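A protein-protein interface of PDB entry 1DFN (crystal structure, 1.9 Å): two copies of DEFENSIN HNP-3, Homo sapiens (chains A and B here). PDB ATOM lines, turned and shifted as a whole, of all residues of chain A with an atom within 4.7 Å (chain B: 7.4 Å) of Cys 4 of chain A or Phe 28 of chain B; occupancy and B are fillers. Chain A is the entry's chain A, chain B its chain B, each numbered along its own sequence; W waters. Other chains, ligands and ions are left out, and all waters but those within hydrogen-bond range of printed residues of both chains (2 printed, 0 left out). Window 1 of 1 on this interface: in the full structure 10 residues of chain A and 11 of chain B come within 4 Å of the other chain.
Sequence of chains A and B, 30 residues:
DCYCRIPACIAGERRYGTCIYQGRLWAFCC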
ATOM      1  N   CYS A   2      22.470  25.701   4.525  1.00  0.00           N
ATOM      2  CA  CYS A   2      21.012  25.654   4.704  1.00  0.00           C
ATOM      3  C   CYS A   2      20.756  24.671   5.882  1.00  0.00           C
ATOM      4  O   CYS A   2      21.463  23.669   6.075  1.00  0.00           O
ATOM      5  CB  CYS A   2      20.254  25.204   3.451  1.00  0.00           C
ATOM      6  SG  CYS A   2      20.276  26.253   2.004  1.00  0.00           S
ATOM      7  N   TYR A   3      19.699  24.990   6.589  1.00  0.00           N
ATOM      8  CA  TYR A   3      19.321  24.172   7.742  1.00  0.00           C
ATOM      9  C   TYR A   3      17.843  23.868   7.753  1.00  0.00           C
ATOM     10  O   TYR A   3      17.162  24.706   7.182  1.00  0.00           O
ATOM     11  CB  TYR A   3      19.474  25.055   9.018  1.00  0.00           C
ATOM     12  CG  TYR A   3      20.903  25.478   9.171  1.00  0.00           C
ATOM     13  CD1 TYR A   3      21.858  24.732   9.830  1.00  0.00           C
ATOM     14  CD2 TYR A   3      21.253  26.665   8.529  1.00  0.00           C
ATOM     15  CE1 TYR A   3      23.191  25.169   9.866  1.00  0.00           C
ATOM     16  CE2 TYR A   3      22.556  27.126   8.552  1.00  0.00           C
ATOM     17  CZ  TYR A   3      23.504  26.366   9.246  1.00  0.00           C
ATOM     18  OH  TYR A   3      24.801  26.835   9.236  1.00  0.00           O
ATOM     19  N   CYS A   4      17.522  22.800   8.461  1.00  0.00           N
ATOM     20  CA  CYS A   4      16.091  22.429   8.678  1.00  0.00           C
ATOM     21  C   CYS A   4      15.821  22.977  10.123  1.00  0.00           C
ATOM     22  O   CYS A   4      16.625  22.625  11.013  1.00  0.00           O
ATOM     23  CB  CYS A   4      15.973  20.923   8.600  1.00  0.00           C
ATOM     24  SG  CYS A   4      16.067  20.394   6.868  1.00  0.00           S
ATOM     25  N   ARG A   5      14.847  23.836  10.296  1.00  0.00           N
ATOM     26  CA  ARG A   5      14.568  24.477  11.581  1.00  0.00           C
ATOM     27  C   ARG A   5      13.128  24.477  11.980  1.00  0.00           C
ATOM     28  O   ARG A   5      12.201  24.534  11.183  1.00  0.00           O
ATOM     29  CB  ARG A   5      14.922  25.962  11.512  1.00  0.00           C
ATOM     30  CG  ARG A   5      16.384  26.225  11.280  1.00  0.00           C
ATOM     31  CD  ARG A   5      16.629  27.668  11.663  1.00  0.00           C
ATOM     32  NE  ARG A   5      17.945  28.096  11.279  1.00  0.00           N
ATOM     33  CZ  ARG A   5      19.037  27.775  11.965  1.00  0.00           C
ATOM     34  NH1 ARG A   5      18.989  27.026  13.091  1.00  0.00           N
ATOM     35  NH2 ARG A   5      20.268  28.146  11.542  1.00  0.00           N
ATOM     36  N   ILE A   6      12.955  24.452  13.305  1.00  0.00           N
ATOM     37  CA  ILE A   6      11.626  24.509  13.983  1.00  0.00           C
ATOM     38  C   ILE A   6      11.890  25.518  15.131  1.00  0.00           C
ATOM     39  O   ILE A   6      12.957  25.419  15.747  1.00  0.00           O
ATOM     40  CB  ILE A   6      11.117  23.144  14.493  1.00  0.00           C
ATOM     41  CG1 ILE A   6      10.433  22.289  13.401  1.00  0.00           C
ATOM     42  CG2 ILE A   6      10.117  23.291  15.713  1.00  0.00           C
ATOM     43  CD1 ILE A   6      10.422  20.757  13.869  1.00  0.00           C
ATOM     44  N   CYS A  19      11.450  20.445   5.338  1.00  0.00           N
ATOM     45  CA  CYS A  19      12.192  19.199   5.531  1.00  0.00           C
ATOM     46  C   CYS A  19      11.258  18.259   6.256  1.00  0.00           C
ATOM     47  O   CYS A  19      10.384  18.742   6.962  1.00  0.00           O
ATOM     48  CB  CYS A  19      13.428  19.297   6.338  1.00  0.00           C
ATOM     49  SG  CYS A  19      14.383  20.817   5.943  1.00  0.00           S
ATOM     50  N   TYR A  21      11.617  15.214   8.854  1.00  0.00           N
ATOM     51  CA  TYR A  21      12.620  14.556   9.698  1.00  0.00           C
ATOM     52  C   TYR A  21      11.977  14.324  11.079  1.00  0.00           C
ATOM     53  O   TYR A  21      11.335  15.235  11.555  1.00  0.00           O
ATOM     54  CB  TYR A  21      13.842  15.431   9.802  1.00  0.00           C
ATOM     55  CG  TYR A  21      14.924  15.088  10.778  1.00  0.00           C
ATOM     56  CD1 TYR A  21      15.641  13.866  10.723  1.00  0.00           C
ATOM     57  CD2 TYR A  21      15.247  16.008  11.763  1.00  0.00           C
ATOM     58  CE1 TYR A  21      16.662  13.588  11.611  1.00  0.00           C
ATOM     59  CE2 TYR A  21      16.274  15.723  12.676  1.00  0.00           C
ATOM     60  CZ  TYR A  21      16.963  14.509  12.600  1.00  0.00           C
ATOM     61  OH  TYR A  21      17.977  14.285  13.479  1.00  0.00           O
ATOM     62  N   TRP A  26       9.775  20.721   9.019  1.00  0.00           N
ATOM     63  CA  TRP A  26      10.767  21.736   9.407  1.00  0.00           C
ATOM     64  C   TRP A  26      10.834  22.771   8.272  1.00  0.00           C
ATOM     65  O   TRP A  26      10.499  22.390   7.136  1.00  0.00           O
ATOM     66  CB  TRP A  26      12.166  21.084   9.506  1.00  0.00           C
ATOM     67  CG  TRP A  26      12.289  19.981  10.479  1.00  0.00           C
ATOM     68  CD1 TRP A  26      11.628  18.772  10.358  1.00  0.00           C
ATOM     69  CD2 TRP A  26      13.033  19.892  11.718  1.00  0.00           C
ATOM     70  NE1 TRP A  26      11.905  17.984  11.460  1.00  0.00           N
ATOM     71  CE2 TRP A  26      12.762  18.634  12.298  1.00  0.00           C
ATOM     72  CE3 TRP A  26      13.864  20.787  12.409  1.00  0.00           C
ATOM     73  CZ2 TRP A  26      13.304  18.201  13.518  1.00  0.00           C
ATOM     74  CZ3 TRP A  26      14.394  20.336  13.629  1.00  0.00           C
ATOM     75  CH2 TRP A  26      14.137  19.089  14.160  1.00  0.00           C
ATOM     76  N   ALA A  27      11.179  23.989   8.534  1.00  0.00           N
ATOM     77  CA  ALA A  27      11.320  24.985   7.492  1.00  0.00           C
ATOM     78  C   ALA A  27      12.710  24.736   6.893  1.00  0.00           C
ATOM     79  O   ALA A  27      13.649  24.491   7.665  1.00  0.00           O
ATOM     80  CB  ALA A  27      11.257  26.383   8.113  1.00  0.00           C
ATOM     81  N   PHE A  28      12.929  24.775   5.598  1.00  0.00           N
ATOM     82  CA  PHE A  28      14.295  24.637   5.043  1.00  0.00           C
ATOM     83  C   PHE A  28      14.688  26.100   4.886  1.00  0.00           C
ATOM     84  O   PHE A  28      14.039  26.857   4.112  1.00  0.00           O
ATOM     85  CB  PHE A  28      14.173  23.830   3.743  1.00  0.00           C
ATOM     86  CG  PHE A  28      15.443  23.743   2.959  1.00  0.00           C
ATOM     87  CD1 PHE A  28      16.529  23.104   3.534  1.00  0.00           C
ATOM     88  CD2 PHE A  28      15.537  24.318   1.678  1.00  0.00           C
ATOM     89  CE1 PHE A  28      17.745  22.989   2.853  1.00  0.00           C
ATOM     90  CE2 PHE A  28      16.757  24.213   0.983  1.00  0.00           C
ATOM     91  CZ  PHE A  28      17.822  23.565   1.583  1.00  0.00           C
ATOM     92  N   ASP B   1      26.498  16.846  12.165  1.00  0.00           N
ATOM     93  CA  ASP B   1      25.252  17.653  12.061  1.00  0.00           C
ATOM     94  C   ASP B   1      24.536  17.095  10.806  1.00  0.00           C
ATOM     95  O   ASP B   1      25.206  16.238  10.135  1.00  0.00           O
ATOM     96  CB  ASP B   1      25.485  19.147  12.091  1.00  0.00           C
ATOM     97  CG  ASP B   1      26.165  19.622  13.415  1.00  0.00           C
ATOM     98  N   CYS B   2      23.323  17.563  10.569  1.00  0.00           N
ATOM     99  CA  CYS B   2      22.547  17.065   9.410  1.00  0.00           C
ATOM    100  C   CYS B   2      22.551  18.029   8.230  1.00  0.00           C
ATOM    101  O   CYS B   2      22.412  19.218   8.491  1.00  0.00           O
ATOM    102  CB  CYS B   2      21.082  16.767   9.786  1.00  0.00           C
ATOM    103  SG  CYS B   2      20.964  15.602  11.171  1.00  0.00           S
ATOM    104  N   TYR B   3      22.660  17.439   7.049  1.00  0.00           N
ATOM    105  CA  TYR B   3      22.671  18.165   5.782  1.00  0.00           C
ATOM    106  C   TYR B   3      21.828  17.525   4.691  1.00  0.00           C
ATOM    107  O   TYR B   3      21.729  16.331   4.666  1.00  0.00           O
ATOM    108  CB  TYR B   3      24.126  18.276   5.251  1.00  0.00           C
ATOM    109  CG  TYR B   3      24.761  19.318   6.145  1.00  0.00           C
ATOM    110  CD1 TYR B   3      24.268  20.636   6.075  1.00  0.00           C
ATOM    111  CD2 TYR B   3      25.749  19.032   7.082  1.00  0.00           C
ATOM    112  CE1 TYR B   3      24.762  21.659   6.887  1.00  0.00           C
ATOM    113  CE2 TYR B   3      26.281  20.037   7.909  1.00  0.00           C
ATOM    114  CZ  TYR B   3      25.783  21.343   7.805  1.00  0.00           C
ATOM    115  OH  TYR B   3      26.316  22.340   8.609  1.00  0.00           O
ATOM    116  N   CYS B   4      21.270  18.348   3.833  1.00  0.00           N
ATOM    117  CA  CYS B   4      20.486  17.899   2.657  1.00  0.00           C
ATOM    118  C   CYS B   4      21.543  17.565   1.597  1.00  0.00           C
ATOM    119  O   CYS B   4      22.432  18.405   1.390  1.00  0.00           O
ATOM    120  CB  CYS B   4      19.699  19.062   2.158  1.00  0.00           C
ATOM    121  SG  CYS B   4      18.395  19.563   3.280  1.00  0.00           S
ATOM    122  N   ARG B   5      21.463  16.398   1.033  1.00  0.00           N
ATOM    123  CA  ARG B   5      22.452  15.935   0.060  1.00  0.00           C
ATOM    124  C   ARG B   5      21.847  15.331  -1.193  1.00  0.00           C
ATOM    125  O   ARG B   5      20.824  14.665  -1.181  1.00  0.00           O
ATOM    126  CB  ARG B   5      23.297  14.782   0.594  1.00  0.00           C
ATOM    127  CG  ARG B   5      23.974  15.043   1.913  1.00  0.00           C
ATOM    128  CD  ARG B   5      25.219  15.811   1.870  1.00  0.00           C
ATOM    129  NE  ARG B   5      25.998  15.641   3.124  1.00  0.00           N
ATOM    130  CZ  ARG B   5      26.849  16.601   3.484  1.00  0.00           C
ATOM    131  NH1 ARG B   5      27.082  17.662   2.712  1.00  0.00           N
ATOM    132  NH2 ARG B   5      27.483  16.674   4.681  1.00  0.00           N
ATOM    133  N   ALA B   8      22.687  11.449  -2.877  1.00  0.00           N
ATOM    134  CA  ALA B   8      22.436  10.646  -1.672  1.00  0.00           C
ATOM    135  C   ALA B   8      23.488  11.019  -0.626  1.00  0.00           C
ATOM    136  O   ALA B   8      24.372  11.857  -0.874  1.00  0.00           O
ATOM    137  CB  ALA B   8      22.418   9.180  -1.967  1.00  0.00           C
ATOM    138  N   CYS B   9      23.307  10.365   0.504  1.00  0.00           N
ATOM    139  CA  CYS B   9      24.211  10.573   1.646  1.00  0.00           C
ATOM    140  C   CYS B   9      25.634  10.089   1.332  1.00  0.00           C
ATOM    141  O   CYS B   9      25.860   9.048   0.718  1.00  0.00           O
ATOM    142  CB  CYS B   9      23.668   9.891   2.908  1.00  0.00           C
ATOM    143  SG  CYS B   9      22.025  10.510   3.466  1.00  0.00           S
ATOM    144  N   GLU B  13      27.313   8.621   6.719  1.00  0.00           N
ATOM    145  CA  GLU B  13      26.110   9.388   7.060  1.00  0.00           C
ATOM    146  C   GLU B  13      24.971   8.437   6.742  1.00  0.00           C
ATOM    147  O   GLU B  13      25.226   7.467   6.017  1.00  0.00           O
ATOM    148  CB  GLU B  13      25.872  10.662   6.321  1.00  0.00           C
ATOM    149  CG  GLU B  13      26.988  11.683   6.402  1.00  0.00           C
ATOM    150  CD  GLU B  13      26.722  12.884   5.550  1.00  0.00           C
ATOM    151  OE1 GLU B  13      25.978  12.700   4.581  1.00  0.00           O
ATOM    152  OE2 GLU B  13      27.243  13.932   5.840  1.00  0.00           O
ATOM    153  N   ARG B  14      23.819   8.700   7.325  1.00  0.00           N
ATOM    154  CA  ARG B  14      22.623   7.895   7.130  1.00  0.00           C
ATOM    155  C   ARG B  14      21.506   8.913   6.804  1.00  0.00           C
ATOM    156  O   ARG B  14      21.546  10.044   7.260  1.00  0.00           O
ATOM    157  CB  ARG B  14      22.154   7.067   8.318  1.00  0.00           C
ATOM    158  CG  ARG B  14      22.729   5.780   8.815  1.00  0.00           C
ATOM    159  CD  ARG B  14      21.995   4.494   8.459  1.00  0.00           C
ATOM    160  N   ARG B  15      20.555   8.415   6.051  1.00  0.00           N
ATOM    161  CA  ARG B  15      19.414   9.149   5.588  1.00  0.00           C
ATOM    162  C   ARG B  15      18.306   9.089   6.653  1.00  0.00           C
ATOM    163  O   ARG B  15      17.863   7.962   6.860  1.00  0.00           O
ATOM    164  CB  ARG B  15      18.804   8.717   4.252  1.00  0.00           C
ATOM    165  CG  ARG B  15      17.799   9.768   3.764  1.00  0.00           C
ATOM    166  CD  ARG B  15      17.070   9.212   2.580  1.00  0.00           C
ATOM    167  NE  ARG B  15      16.143  10.165   2.006  1.00  0.00           N
ATOM    168  CZ  ARG B  15      15.726  10.393   0.757  1.00  0.00           C
ATOM    169  NH1 ARG B  15      16.250   9.640  -0.261  1.00  0.00           N
ATOM    170  NH2 ARG B  15      14.839  11.351   0.408  1.00  0.00           N
ATOM    171  N   TYR B  16      17.967  10.222   7.188  1.00  0.00           N
ATOM    172  CA  TYR B  16      16.914  10.276   8.220  1.00  0.00           C
ATOM    173  C   TYR B  16      15.716  11.086   7.742  1.00  0.00           C
ATOM    174  O   TYR B  16      14.677  11.194   8.462  1.00  0.00           O
ATOM    175  CB  TYR B  16      17.520  10.929   9.483  1.00  0.00           C
ATOM    176  CG  TYR B  16      18.491  10.026  10.164  1.00  0.00           C
ATOM    177  CD1 TYR B  16      18.038   8.937  10.885  1.00  0.00           C
ATOM    178  CD2 TYR B  16      19.876  10.260  10.113  1.00  0.00           C
ATOM    179  CE1 TYR B  16      18.957   8.085  11.528  1.00  0.00           C
ATOM    180  CE2 TYR B  16      20.768   9.455  10.775  1.00  0.00           C
ATOM    181  CZ  TYR B  16      20.301   8.339  11.475  1.00  0.00           C
ATOM    182  OH  TYR B  16      21.155   7.495  12.132  1.00  0.00           O
ATOM    183  N   GLY B  17      15.767  11.689   6.559  1.00  0.00           N
ATOM    184  CA  GLY B  17      14.670  12.503   6.093  1.00  0.00           C
ATOM    185  C   GLY B  17      14.860  13.002   4.666  1.00  0.00           C
ATOM    186  O   GLY B  17      15.671  12.461   3.908  1.00  0.00           O
ATOM    187  N   THR B  18      14.088  14.012   4.341  1.00  0.00           N
ATOM    188  CA  THR B  18      14.059  14.614   3.019  1.00  0.00           C
ATOM    189  C   THR B  18      13.944  16.121   3.101  1.00  0.00           C
ATOM    190  O   THR B  18      13.208  16.607   3.987  1.00  0.00           O
ATOM    191  CB  THR B  18      12.750  14.157   2.239  1.00  0.00           C
ATOM    192  OG1 THR B  18      12.688  12.718   2.348  1.00  0.00           O
ATOM    193  CG2 THR B  18      12.671  14.534   0.752  1.00  0.00           C
ATOM    194  N   CYS B  19      14.630  16.769   2.182  1.00  0.00           N
ATOM    195  CA  CYS B  19      14.540  18.223   2.071  1.00  0.00           C
ATOM    196  C   CYS B  19      13.840  18.469   0.713  1.00  0.00           C
ATOM    197  O   CYS B  19      14.227  17.865  -0.302  1.00  0.00           O
ATOM    198  CB  CYS B  19      15.820  18.886   2.095  1.00  0.00           C
ATOM    199  SG  CYS B  19      16.986  18.174   3.244  1.00  0.00           S
ATOM    200  N   ILE B  20      12.811  19.245   0.762  1.00  0.00           N
ATOM    201  CA  ILE B  20      12.004  19.536  -0.411  1.00  0.00           C
ATOM    202  C   ILE B  20      12.282  20.961  -0.809  1.00  0.00           C
ATOM    203  O   ILE B  20      12.015  21.850  -0.013  1.00  0.00           O
ATOM    204  CB  ILE B  20      10.483  19.279  -0.082  1.00  0.00           C
ATOM    205  CG1 ILE B  20      10.366  17.813   0.441  1.00  0.00           C
ATOM    206  CG2 ILE B  20       9.588  19.441  -1.312  1.00  0.00           C
ATOM    207  CD1 ILE B  20       8.929  17.664   0.968  1.00  0.00           C
ATOM    208  N   LEU B  25      13.493  16.632  -4.365  1.00  0.00           N
ATOM    209  CA  LEU B  25      13.623  15.976  -3.076  1.00  0.00           C
ATOM    210  C   LEU B  25      15.083  15.625  -2.842  1.00  0.00           C
ATOM    211  O   LEU B  25      15.594  14.854  -3.681  1.00  0.00           O
ATOM    212  CB  LEU B  25      12.790  14.705  -3.000  1.00  0.00           C
ATOM    213  CG  LEU B  25      11.299  14.819  -3.182  1.00  0.00           C
ATOM    214  CD1 LEU B  25      10.784  13.383  -3.080  1.00  0.00           C
ATOM    215  CD2 LEU B  25      10.632  15.516  -2.013  1.00  0.00           C
ATOM    216  N   TRP B  26      15.728  16.139  -1.831  1.00  0.00           N
ATOM    217  CA  TRP B  26      17.081  15.841  -1.421  1.00  0.00           C
ATOM    218  C   TRP B  26      17.055  14.973  -0.155  1.00  0.00           C
ATOM    219  O   TRP B  26      16.112  14.982   0.666  1.00  0.00           O
ATOM    220  CB  TRP B  26      17.753  17.175  -1.128  1.00  0.00           C
ATOM    221  CG  TRP B  26      17.774  18.036  -2.358  1.00  0.00           C
ATOM    222  CD1 TRP B  26      17.801  17.587  -3.668  1.00  0.00           C
ATOM    223  CD2 TRP B  26      17.810  19.456  -2.408  1.00  0.00           C
ATOM    224  NE1 TRP B  26      17.842  18.679  -4.524  1.00  0.00           N
ATOM    225  CE2 TRP B  26      17.851  19.832  -3.769  1.00  0.00           C
ATOM    226  CE3 TRP B  26      17.823  20.432  -1.407  1.00  0.00           C
ATOM    227  CZ2 TRP B  26      17.908  21.148  -4.204  1.00  0.00           C
ATOM    228  CZ3 TRP B  26      17.856  21.760  -1.812  1.00  0.00           C
ATOM    229  CH2 TRP B  26      17.914  22.100  -3.190  1.00  0.00           C
ATOM    230  N   ALA B  27      18.080  14.196   0.024  1.00  0.00           N
ATOM    231  CA  ALA B  27      18.315  13.326   1.176  1.00  0.00           C
ATOM    232  C   ALA B  27      18.731  14.232   2.348  1.00  0.00           C
ATOM    233  O   ALA B  27      19.581  15.117   2.136  1.00  0.00           O
ATOM    234  CB  ALA B  27      19.445  12.360   0.929  1.00  0.00           C
ATOM    235  N   PHE B  28      18.113  13.934   3.503  1.00  0.00           N
ATOM    236  CA  PHE B  28      18.461  14.679   4.734  1.00  0.00           C
ATOM    237  C   PHE B  28      19.374  13.660   5.420  1.00  0.00           C
ATOM    238  O   PHE B  28      18.822  12.634   5.785  1.00  0.00           O
ATOM    239  CB  PHE B  28      17.295  15.075   5.603  1.00  0.00           C
ATOM    240  CG  PHE B  28      17.693  15.990   6.735  1.00  0.00           C
ATOM    241  CD1 PHE B  28      18.368  17.199   6.437  1.00  0.00           C
ATOM    242  CD2 PHE B  28      17.367  15.654   8.039  1.00  0.00           C
ATOM    243  CE1 PHE B  28      18.770  18.090   7.442  1.00  0.00           C
ATOM    244  CE2 PHE B  28      17.760  16.571   9.068  1.00  0.00           C
ATOM    245  CZ  PHE B  28      18.431  17.767   8.778  1.00  0.00           C
ATOM    246  N   CYS B  29      20.622  13.872   5.542  1.00  0.00           N
ATOM    247  CA  CYS B  29      21.628  12.985   6.064  1.00  0.00           C
ATOM    248  C   CYS B  29      22.334  13.448   7.342  1.00  0.00           C
ATOM    249  O   CYS B  29      22.820  14.594   7.307  1.00  0.00           O
ATOM    250  CB  CYS B  29      22.775  12.998   4.991  1.00  0.00           C
ATOM    251  SG  CYS B  29      22.104  12.467   3.379  1.00  0.00           S
ATOM    252  N   CYS B  30      22.443  12.482   8.240  1.00  0.00           N
ATOM    253  CA  CYS B  30      23.133  12.837   9.509  1.00  0.00           C
ATOM    254  C   CYS B  30      24.317  11.923   9.713  1.00  0.00           C
ATOM    255  O   CYS B  30      24.259  10.774   9.281  1.00  0.00           O
ATOM    256  CB  CYS B  30      22.142  12.817  10.692  1.00  0.00           C
ATOM    257  SG  CYS B  30      20.631  13.764  10.425  1.00  0.00           S
ATOM    258  OXT CYS B  30      25.294  12.409  10.285  1.00  0.00           O
HETATM  259  O   HOH W   1      21.556  21.436   4.330  1.00  0.00           O
HETATM  260  O   HOH W   2      21.370  21.540   7.482  1.00  0.00           O
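Of the 10 printed residues of chain A, 5 touch a printed residue of chain B. Of the 21 printed residues of chain B, 7 touch a printed residue of chain A. Among the printed residues, 8 pairs touch across the chains. Among the printed residues, no Asp or Glu carboxylate lies within 4 Å of a Lys or Arg side-chain nitrogen of the other chain.
Cys 4 of chain A touches just one residue of chain B: Phe 28 (3.6 Å). Of the printed residues of chain A, Tyr 3 of chain B touches Cys 2. Printed residues of chain A within 4 Å of Cys 4 of chain B: Phe 28 (3.5 Å). Of the printed residues of chain A, Thr 18 of chain B touches Cys 19 (3.2 Å). Of the printed residues of chain B, Cys 2 of chain A touches Tyr 3. Of the printed residues of chain A, Trp 26 of chain B touches Phe 28 (3.8 Å). The nearest printed residue of chain A that does not touch Phe 28 of chain B is Cys 19 of chain A (5.4 Å).
Cys 2 of chain A touches Tyr 3 of chain B. SG of Cys 4 of chain A touches CE1 of Phe 28 of chain B, 3.6 Å away. Cys 19 of chain A touches Thr 18 of chain B. OH of Tyr 21 of chain A touches SG of Cys 2 of chain B, 3.998 Å away. Tyr 16 of chain B touches Tyr 21 of chain A (CB to CE1, 3.5 Å). Tyr 21 of chain A touches Phe 28 of chain B. Cys 4 of chain B touches Phe 28 of chain A (SG to CE1, 3.5 Å). Phe 28 of chain A touches Trp 26 of chain B.
The side-chain sulfur (SG) of Cys 19 of chain A forms a disulfide with the side-chain sulfur (SG) of Cys 4 of chain A (2.0 Å). O of Tyr 3 of chain B sits at hydrogen-bond distance from N of Cys 29 of chain B (2.8 Å). The backbone NH of Tyr 16 of chain B lies within hydrogen-bond range of the backbone carbonyl oxygen of Phe 28 of chain B, 2.9 Å away. O of Gly 17 of chain B lies within hydrogen-bond range of N of Phe 28 of chain B. The backbone carbonyl oxygen (O) of Cys 19 of chain B sits at hydrogen-bond distance from the backbone NH (N) of Trp 26 of chain B, at 2.8 Å. The side-chain sulfur of Cys 9 of chain B is disulfide-bonded to the side-chain sulfur of Cys 29 of chain B.
Cys 2 of chain A touches Tyr 3 of chain B, but with the chains exchanged Tyr 3 of chain A does not touch Cys 2 of chain B (5.7 Å). Cys 4 of chain A touches Phe 28 of chain B, and with the chains exchanged Phe 28 of chain A touches Cys 4 of chain B. Phe 28 of chain A touches Trp 26 of chain B, but with the chains exchanged Trp 26 of chain A does not touch Phe 28 of chain B (6.3 Å). 8 positions are printed for both chains. Of the 8 pairs that touch across the chains among the printed residues, 2 have their exchanged pair printed and touching as well.
Water W2 bridges O of Cys 2 of chain A (2.6 Å) and O of Cys 2 of chain B (2.7 Å). Water W1 bridges O of Cys 2 of chain A and N of Cys 4 of chain B.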
